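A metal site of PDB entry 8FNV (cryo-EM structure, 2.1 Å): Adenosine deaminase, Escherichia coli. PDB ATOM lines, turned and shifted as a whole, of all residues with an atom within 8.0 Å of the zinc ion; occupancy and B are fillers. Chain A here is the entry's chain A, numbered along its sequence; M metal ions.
A ring nitrogen (NE2) of His 154 lies close to the side-chain carboxylate (OD2) of Asp 748 (3.2 Å).
OD1 of Asp 467 lies within hydrogen-bond range of ND1 of His 498 (3.2 Å).
The backbone carbonyl oxygen (O) of Ala 468 sits at hydrogen-bond distance from the backbone NH (N) of His 498 (3.0 Å).
A ring nitrogen (ND1) of His 152 sits close to the guanidinium group of Arg 356, 3.4 Å away.
ND1 of His 152 is in hydrogen-bond range of OE1 of Glu 704, 2.7 Å away.
The zinc ion is bound by NE2 of His 154 (2.2 Å), NE2 of His 530 (2.2 Å), NE2 of His 498 (2.3 Å) and NE2 of His 152 (2.3 Å).
The zinc ion has four donor atoms within binding distance.
Residues that only touch the zinc ion: Glu 501 (3.8 Å).
Five residues have an atom within 4 Å of the zinc ion: His 152, His 154, His 498, Glu 501 and His 530.
The nearest printed residue that does not touch the zinc ion is Asp 748 (4.4 Å).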
ATOM      1  N   HIS A 152     -33.904  -2.236  27.986  1.00  0.00           N
ATOM      2  CA  HIS A 152     -33.557  -1.940  26.597  1.00  0.00           C
ATOM      3  C   HIS A 152     -34.835  -1.974  25.766  1.00  0.00           C
ATOM      4  O   HIS A 152     -35.276  -3.050  25.333  1.00  0.00           O
ATOM      5  CB  HIS A 152     -32.529  -2.936  26.073  1.00  0.00           C
ATOM      6  CG  HIS A 152     -31.573  -2.355  25.075  1.00  0.00           C
ATOM      7  ND1 HIS A 152     -30.629  -1.414  25.403  1.00  0.00           N
ATOM      8  CD2 HIS A 152     -31.431  -2.580  23.752  1.00  0.00           C
ATOM      9  CE1 HIS A 152     -29.933  -1.098  24.335  1.00  0.00           C
ATOM     10  NE2 HIS A 152     -30.405  -1.779  23.313  1.00  0.00           N
ATOM     11  N   GLN A 153     -35.431  -0.794  25.536  1.00  0.00           N
ATOM     12  CA  GLN A 153     -36.651  -0.691  24.734  1.00  0.00           C
ATOM     13  C   GLN A 153     -36.600   0.587  23.893  1.00  0.00           C
ATOM     14  O   GLN A 153     -37.051   1.649  24.349  1.00  0.00           O
ATOM     15  CB  GLN A 153     -37.875  -0.702  25.643  1.00  0.00           C
ATOM     16  CG  GLN A 153     -38.921  -1.733  25.267  1.00  0.00           C
ATOM     17  CD  GLN A 153     -40.250  -1.468  25.929  1.00  0.00           C
ATOM     18  OE1 GLN A 153     -40.316  -0.920  27.026  1.00  0.00           O
ATOM     19  NE2 GLN A 153     -41.331  -1.848  25.256  1.00  0.00           N
ATOM     20  N   HIS A 154     -36.028   0.514  22.693  1.00  0.00           N
ATOM     21  CA  HIS A 154     -35.773   1.616  21.766  1.00  0.00           C
ATOM     22  C   HIS A 154     -35.920   1.256  20.287  1.00  0.00           C
ATOM     23  O   HIS A 154     -35.316   1.928  19.449  1.00  0.00           O
ATOM     24  CB  HIS A 154     -34.388   2.182  22.038  1.00  0.00           C
ATOM     25  CG  HIS A 154     -33.281   1.338  21.522  1.00  0.00           C
ATOM     26  ND1 HIS A 154     -32.753   1.514  20.257  1.00  0.00           N
ATOM     27  CD2 HIS A 154     -32.629   0.290  22.068  1.00  0.00           C
ATOM     28  CE1 HIS A 154     -31.798   0.619  20.065  1.00  0.00           C
ATOM     29  NE2 HIS A 154     -31.713  -0.144  21.132  1.00  0.00           N
ATOM     30  N   LEU A 155     -36.699   0.219  19.924  1.00  0.00           N
ATOM     31  CA  LEU A 155     -36.630  -0.294  18.546  1.00  0.00           C
ATOM     32  C   LEU A 155     -37.584   0.400  17.570  1.00  0.00           C
ATOM     33  O   LEU A 155     -37.103   1.034  16.637  1.00  0.00           O
ATOM     34  CB  LEU A 155     -36.891  -1.803  18.514  1.00  0.00           C
ATOM     35  CG  LEU A 155     -35.696  -2.758  18.258  1.00  0.00           C
ATOM     36  CD1 LEU A 155     -36.175  -4.196  18.013  1.00  0.00           C
ATOM     37  CD2 LEU A 155     -34.581  -2.314  17.295  1.00  0.00           C
ATOM     38  N   ARG A 356     -37.052   4.801  26.756  1.00  0.00           N
ATOM     39  CA  ARG A 356     -36.052   5.526  25.982  1.00  0.00           C
ATOM     40  C   ARG A 356     -36.731   6.315  24.867  1.00  0.00           C
ATOM     41  O   ARG A 356     -37.537   5.761  24.117  1.00  0.00           O
ATOM     42  CB  ARG A 356     -35.010   4.561  25.409  1.00  0.00           C
ATOM     43  CG  ARG A 356     -33.995   4.127  26.430  1.00  0.00           C
ATOM     44  CD  ARG A 356     -32.974   3.169  25.854  1.00  0.00           C
ATOM     45  NE  ARG A 356     -32.310   2.425  26.921  1.00  0.00           N
ATOM     46  CZ  ARG A 356     -31.120   1.856  26.818  1.00  0.00           C
ATOM     47  NH1 ARG A 356     -30.422   1.924  25.694  1.00  0.00           N
ATOM     48  NH2 ARG A 356     -30.614   1.214  27.865  1.00  0.00           N
ATOM     49  N   HIS A 421     -32.265   9.456  24.327  1.00  0.00           N
ATOM     50  CA  HIS A 421     -31.290   8.954  23.378  1.00  0.00           C
ATOM     51  C   HIS A 421     -30.257  10.028  23.050  1.00  0.00           C
ATOM     52  O   HIS A 421     -30.293  11.152  23.556  1.00  0.00           O
ATOM     53  CB  HIS A 421     -31.967   8.536  22.072  1.00  0.00           C
ATOM     54  CG  HIS A 421     -32.565   7.164  22.100  1.00  0.00           C
ATOM     55  ND1 HIS A 421     -32.048   6.132  22.859  1.00  0.00           N
ATOM     56  CD2 HIS A 421     -33.636   6.651  21.444  1.00  0.00           C
ATOM     57  CE1 HIS A 421     -32.781   5.052  22.677  1.00  0.00           C
ATOM     58  NE2 HIS A 421     -33.744   5.343  21.824  1.00  0.00           N
ATOM     59  N   ASP A 467     -28.623   7.733  27.197  1.00  0.00           N
ATOM     60  CA  ASP A 467     -28.108   6.698  26.304  1.00  0.00           C
ATOM     61  C   ASP A 467     -27.776   7.310  24.950  1.00  0.00           C
ATOM     62  O   ASP A 467     -28.489   8.193  24.464  1.00  0.00           O
ATOM     63  CB  ASP A 467     -29.125   5.580  26.136  1.00  0.00           C
ATOM     64  CG  ASP A 467     -28.759   4.622  25.017  1.00  0.00           C
ATOM     65  OD1 ASP A 467     -27.675   4.007  25.086  1.00  0.00           O
ATOM     66  OD2 ASP A 467     -29.565   4.484  24.065  1.00  0.00           O
ATOM     67  N   ALA A 468     -26.679   6.851  24.354  1.00  0.00           N
ATOM     68  CA  ALA A 468     -26.359   7.207  22.970  1.00  0.00           C
ATOM     69  C   ALA A 468     -26.464   5.933  22.136  1.00  0.00           C
ATOM     70  O   ALA A 468     -25.579   5.068  22.161  1.00  0.00           O
ATOM     71  CB  ALA A 468     -24.986   7.837  22.853  1.00  0.00           C
ATOM     72  N   ALA A 469     -27.589   5.809  21.427  1.00  0.00           N
ATOM     73  CA  ALA A 469     -27.834   4.713  20.492  1.00  0.00           C
ATOM     74  C   ALA A 469     -27.571   5.215  19.074  1.00  0.00           C
ATOM     75  O   ALA A 469     -26.970   6.276  18.890  1.00  0.00           O
ATOM     76  CB  ALA A 469     -29.253   4.163  20.633  1.00  0.00           C
ATOM     77  N   ALA A 470     -28.017   4.448  18.078  1.00  0.00           N
ATOM     78  CA  ALA A 470     -27.867   4.638  16.639  1.00  0.00           C
ATOM     79  C   ALA A 470     -26.637   3.876  16.173  1.00  0.00           C
ATOM     80  O   ALA A 470     -26.016   3.146  16.957  1.00  0.00           O
ATOM     81  CB  ALA A 470     -27.774   6.128  16.270  1.00  0.00           C
ATOM     82  N   TYR A 497     -24.450   3.577  26.465  1.00  0.00           N
ATOM     83  CA  TYR A 497     -23.854   3.814  25.149  1.00  0.00           C
ATOM     84  C   TYR A 497     -23.801   2.505  24.375  1.00  0.00           C
ATOM     85  O   TYR A 497     -23.155   1.555  24.823  1.00  0.00           O
ATOM     86  CB  TYR A 497     -22.462   4.424  25.292  1.00  0.00           C
ATOM     87  CG  TYR A 497     -21.893   4.908  23.987  1.00  0.00           C
ATOM     88  CD1 TYR A 497     -21.523   4.010  23.004  1.00  0.00           C
ATOM     89  CD2 TYR A 497     -21.748   6.256  23.727  1.00  0.00           C
ATOM     90  CE1 TYR A 497     -21.006   4.433  21.805  1.00  0.00           C
ATOM     91  CE2 TYR A 497     -21.230   6.697  22.527  1.00  0.00           C
ATOM     92  CZ  TYR A 497     -20.867   5.783  21.568  1.00  0.00           C
ATOM     93  OH  TYR A 497     -20.350   6.207  20.369  1.00  0.00           O
ATOM     94  N   HIS A 498     -24.439   2.465  23.217  1.00  0.00           N
ATOM     95  CA  HIS A 498     -24.411   1.264  22.394  1.00  0.00           C
ATOM     96  C   HIS A 498     -23.012   1.013  21.859  1.00  0.00           C
ATOM     97  O   HIS A 498     -22.417   1.889  21.207  1.00  0.00           O
ATOM     98  CB  HIS A 498     -25.398   1.410  21.238  1.00  0.00           C
ATOM     99  CG  HIS A 498     -26.821   1.189  21.631  1.00  0.00           C
ATOM    100  ND1 HIS A 498     -27.461   1.975  22.563  1.00  0.00           N
ATOM    101  CD2 HIS A 498     -27.730   0.263  21.227  1.00  0.00           C
ATOM    102  CE1 HIS A 498     -28.707   1.547  22.709  1.00  0.00           C
ATOM    103  NE2 HIS A 498     -28.891   0.513  21.916  1.00  0.00           N
ATOM    104  N   VAL A 499     -22.471  -0.178  22.126  1.00  0.00           N
ATOM    105  CA  VAL A 499     -21.150  -0.565  21.641  1.00  0.00           C
ATOM    106  C   VAL A 499     -21.175  -2.025  21.248  1.00  0.00           C
ATOM    107  O   VAL A 499     -21.915  -2.844  21.821  1.00  0.00           O
ATOM    108  CB  VAL A 499     -20.045  -0.313  22.703  1.00  0.00           C
ATOM    109  CG1 VAL A 499     -19.647   1.140  22.727  1.00  0.00           C
ATOM    110  CG2 VAL A 499     -20.500  -0.777  24.077  1.00  0.00           C
ATOM    111  N   GLU A 501     -22.253  -3.511  18.542  1.00  0.00           N
ATOM    112  CA  GLU A 501     -23.349  -4.026  17.731  1.00  0.00           C
ATOM    113  C   GLU A 501     -22.892  -4.355  16.302  1.00  0.00           C
ATOM    114  O   GLU A 501     -22.911  -5.521  15.887  1.00  0.00           O
ATOM    115  CB  GLU A 501     -24.498  -3.016  17.708  1.00  0.00           C
ATOM    116  CG  GLU A 501     -25.650  -3.392  18.605  1.00  0.00           C
ATOM    117  CD  GLU A 501     -26.955  -2.761  18.179  1.00  0.00           C
ATOM    118  OE1 GLU A 501     -27.782  -3.468  17.559  1.00  0.00           O
ATOM    119  OE2 GLU A 501     -27.167  -1.563  18.473  1.00  0.00           O
ATOM    120  N   LEU A 528     -23.621  -0.646  29.494  1.00  0.00           N
ATOM    121  CA  LEU A 528     -23.106  -0.240  28.186  1.00  0.00           C
ATOM    122  C   LEU A 528     -24.138  -0.441  27.080  1.00  0.00           C
ATOM    123  O   LEU A 528     -24.595   0.526  26.468  1.00  0.00           O
ATOM    124  CB  LEU A 528     -21.825  -1.014  27.861  1.00  0.00           C
ATOM    125  CG  LEU A 528     -20.516  -0.238  28.071  1.00  0.00           C
ATOM    126  CD1 LEU A 528     -19.323  -1.102  27.701  1.00  0.00           C
ATOM    127  CD2 LEU A 528     -20.505   1.057  27.278  1.00  0.00           C
ATOM    128  N   GLY A 529     -24.549  -1.675  26.836  1.00  0.00           N
ATOM    129  CA  GLY A 529     -25.417  -1.959  25.702  1.00  0.00           C
ATOM    130  C   GLY A 529     -25.315  -3.387  25.221  1.00  0.00           C
ATOM    131  O   GLY A 529     -25.220  -4.312  26.020  1.00  0.00           O
ATOM    132  N   HIS A 530     -25.315  -3.574  23.891  1.00  0.00           N
ATOM    133  CA  HIS A 530     -25.291  -4.915  23.332  1.00  0.00           C
ATOM    134  C   HIS A 530     -23.956  -5.599  23.576  1.00  0.00           C
ATOM    135  O   HIS A 530     -23.907  -6.738  24.060  1.00  0.00           O
ATOM    136  CB  HIS A 530     -25.610  -4.864  21.839  1.00  0.00           C
ATOM    137  CG  HIS A 530     -26.986  -4.378  21.520  1.00  0.00           C
ATOM    138  ND1 HIS A 530     -27.839  -5.073  20.694  1.00  0.00           N
ATOM    139  CD2 HIS A 530     -27.654  -3.270  21.916  1.00  0.00           C
ATOM    140  CE1 HIS A 530     -28.981  -4.410  20.602  1.00  0.00           C
ATOM    141  NE2 HIS A 530     -28.894  -3.315  21.332  1.00  0.00           N
ATOM    142  N   GLU A 704     -26.619  -4.849  28.735  1.00  0.00           N
ATOM    143  CA  GLU A 704     -27.987  -5.147  28.307  1.00  0.00           C
ATOM    144  C   GLU A 704     -27.909  -5.974  27.028  1.00  0.00           C
ATOM    145  O   GLU A 704     -27.473  -5.471  25.988  1.00  0.00           O
ATOM    146  CB  GLU A 704     -28.821  -3.887  28.082  1.00  0.00           C
ATOM    147  CG  GLU A 704     -28.698  -2.783  29.096  1.00  0.00           C
ATOM    148  CD  GLU A 704     -28.860  -1.373  28.566  1.00  0.00           C
ATOM    149  OE1 GLU A 704     -28.782  -1.136  27.329  1.00  0.00           O
ATOM    150  OE2 GLU A 704     -29.031  -0.468  29.405  1.00  0.00           O
ATOM    151  N   PRO A 706     -30.241  -7.891  24.500  1.00  0.00           N
ATOM    152  CA  PRO A 706     -31.493  -8.375  23.930  1.00  0.00           C
ATOM    153  C   PRO A 706     -31.223  -9.454  22.902  1.00  0.00           C
ATOM    154  O   PRO A 706     -30.083  -9.624  22.450  1.00  0.00           O
ATOM    155  CB  PRO A 706     -32.095  -7.115  23.287  1.00  0.00           C
ATOM    156  CG  PRO A 706     -30.925  -6.241  22.959  1.00  0.00           C
ATOM    157  CD  PRO A 706     -29.745  -6.694  23.788  1.00  0.00           C
ATOM    158  N   THR A 708     -31.043 -11.027  19.333  1.00  0.00           N
ATOM    159  CA  THR A 708     -30.989 -10.589  17.946  1.00  0.00           C
ATOM    160  C   THR A 708     -30.944 -11.782  17.000  1.00  0.00           C
ATOM    161  O   THR A 708     -29.911 -12.059  16.378  1.00  0.00           O
ATOM    162  CB  THR A 708     -29.755  -9.692  17.688  1.00  0.00           C
ATOM    163  OG1 THR A 708     -28.566 -10.497  17.705  1.00  0.00           O
ATOM    164  CG2 THR A 708     -29.638  -8.608  18.747  1.00  0.00           C
ATOM    165  N   ASP A 748     -35.868  -6.267  22.918  1.00  0.00           N
ATOM    166  CA  ASP A 748     -35.564  -5.618  21.651  1.00  0.00           C
ATOM    167  C   ASP A 748     -35.177  -6.710  20.649  1.00  0.00           C
ATOM    168  O   ASP A 748     -34.023  -7.155  20.625  1.00  0.00           O
ATOM    169  CB  ASP A 748     -34.455  -4.594  21.811  1.00  0.00           C
ATOM    170  CG  ASP A 748     -34.957  -3.166  21.751  1.00  0.00           C
ATOM    171  OD1 ASP A 748     -36.179  -2.953  21.878  1.00  0.00           O
ATOM    172  OD2 ASP A 748     -34.129  -2.253  21.590  1.00  0.00           O
ATOM    173  N   PRO A 750     -34.894  -7.217  16.704  1.00  0.00           N
ATOM    174  CA  PRO A 750     -34.972  -6.401  15.478  1.00  0.00           C
ATOM    175  C   PRO A 750     -35.984  -6.900  14.460  1.00  0.00           C
ATOM    176  O   PRO A 750     -36.640  -6.073  13.800  1.00  0.00           O
ATOM    177  CB  PRO A 750     -33.545  -6.474  14.928  1.00  0.00           C
ATOM    178  CG  PRO A 750     -32.691  -6.766  16.112  1.00  0.00           C
ATOM    179  CD  PRO A 750     -33.522  -7.652  16.993  1.00  0.00           C
HETATM  180 ZN    ZN M   1     -29.901  -1.348  21.096  1.00  0.00          ZN
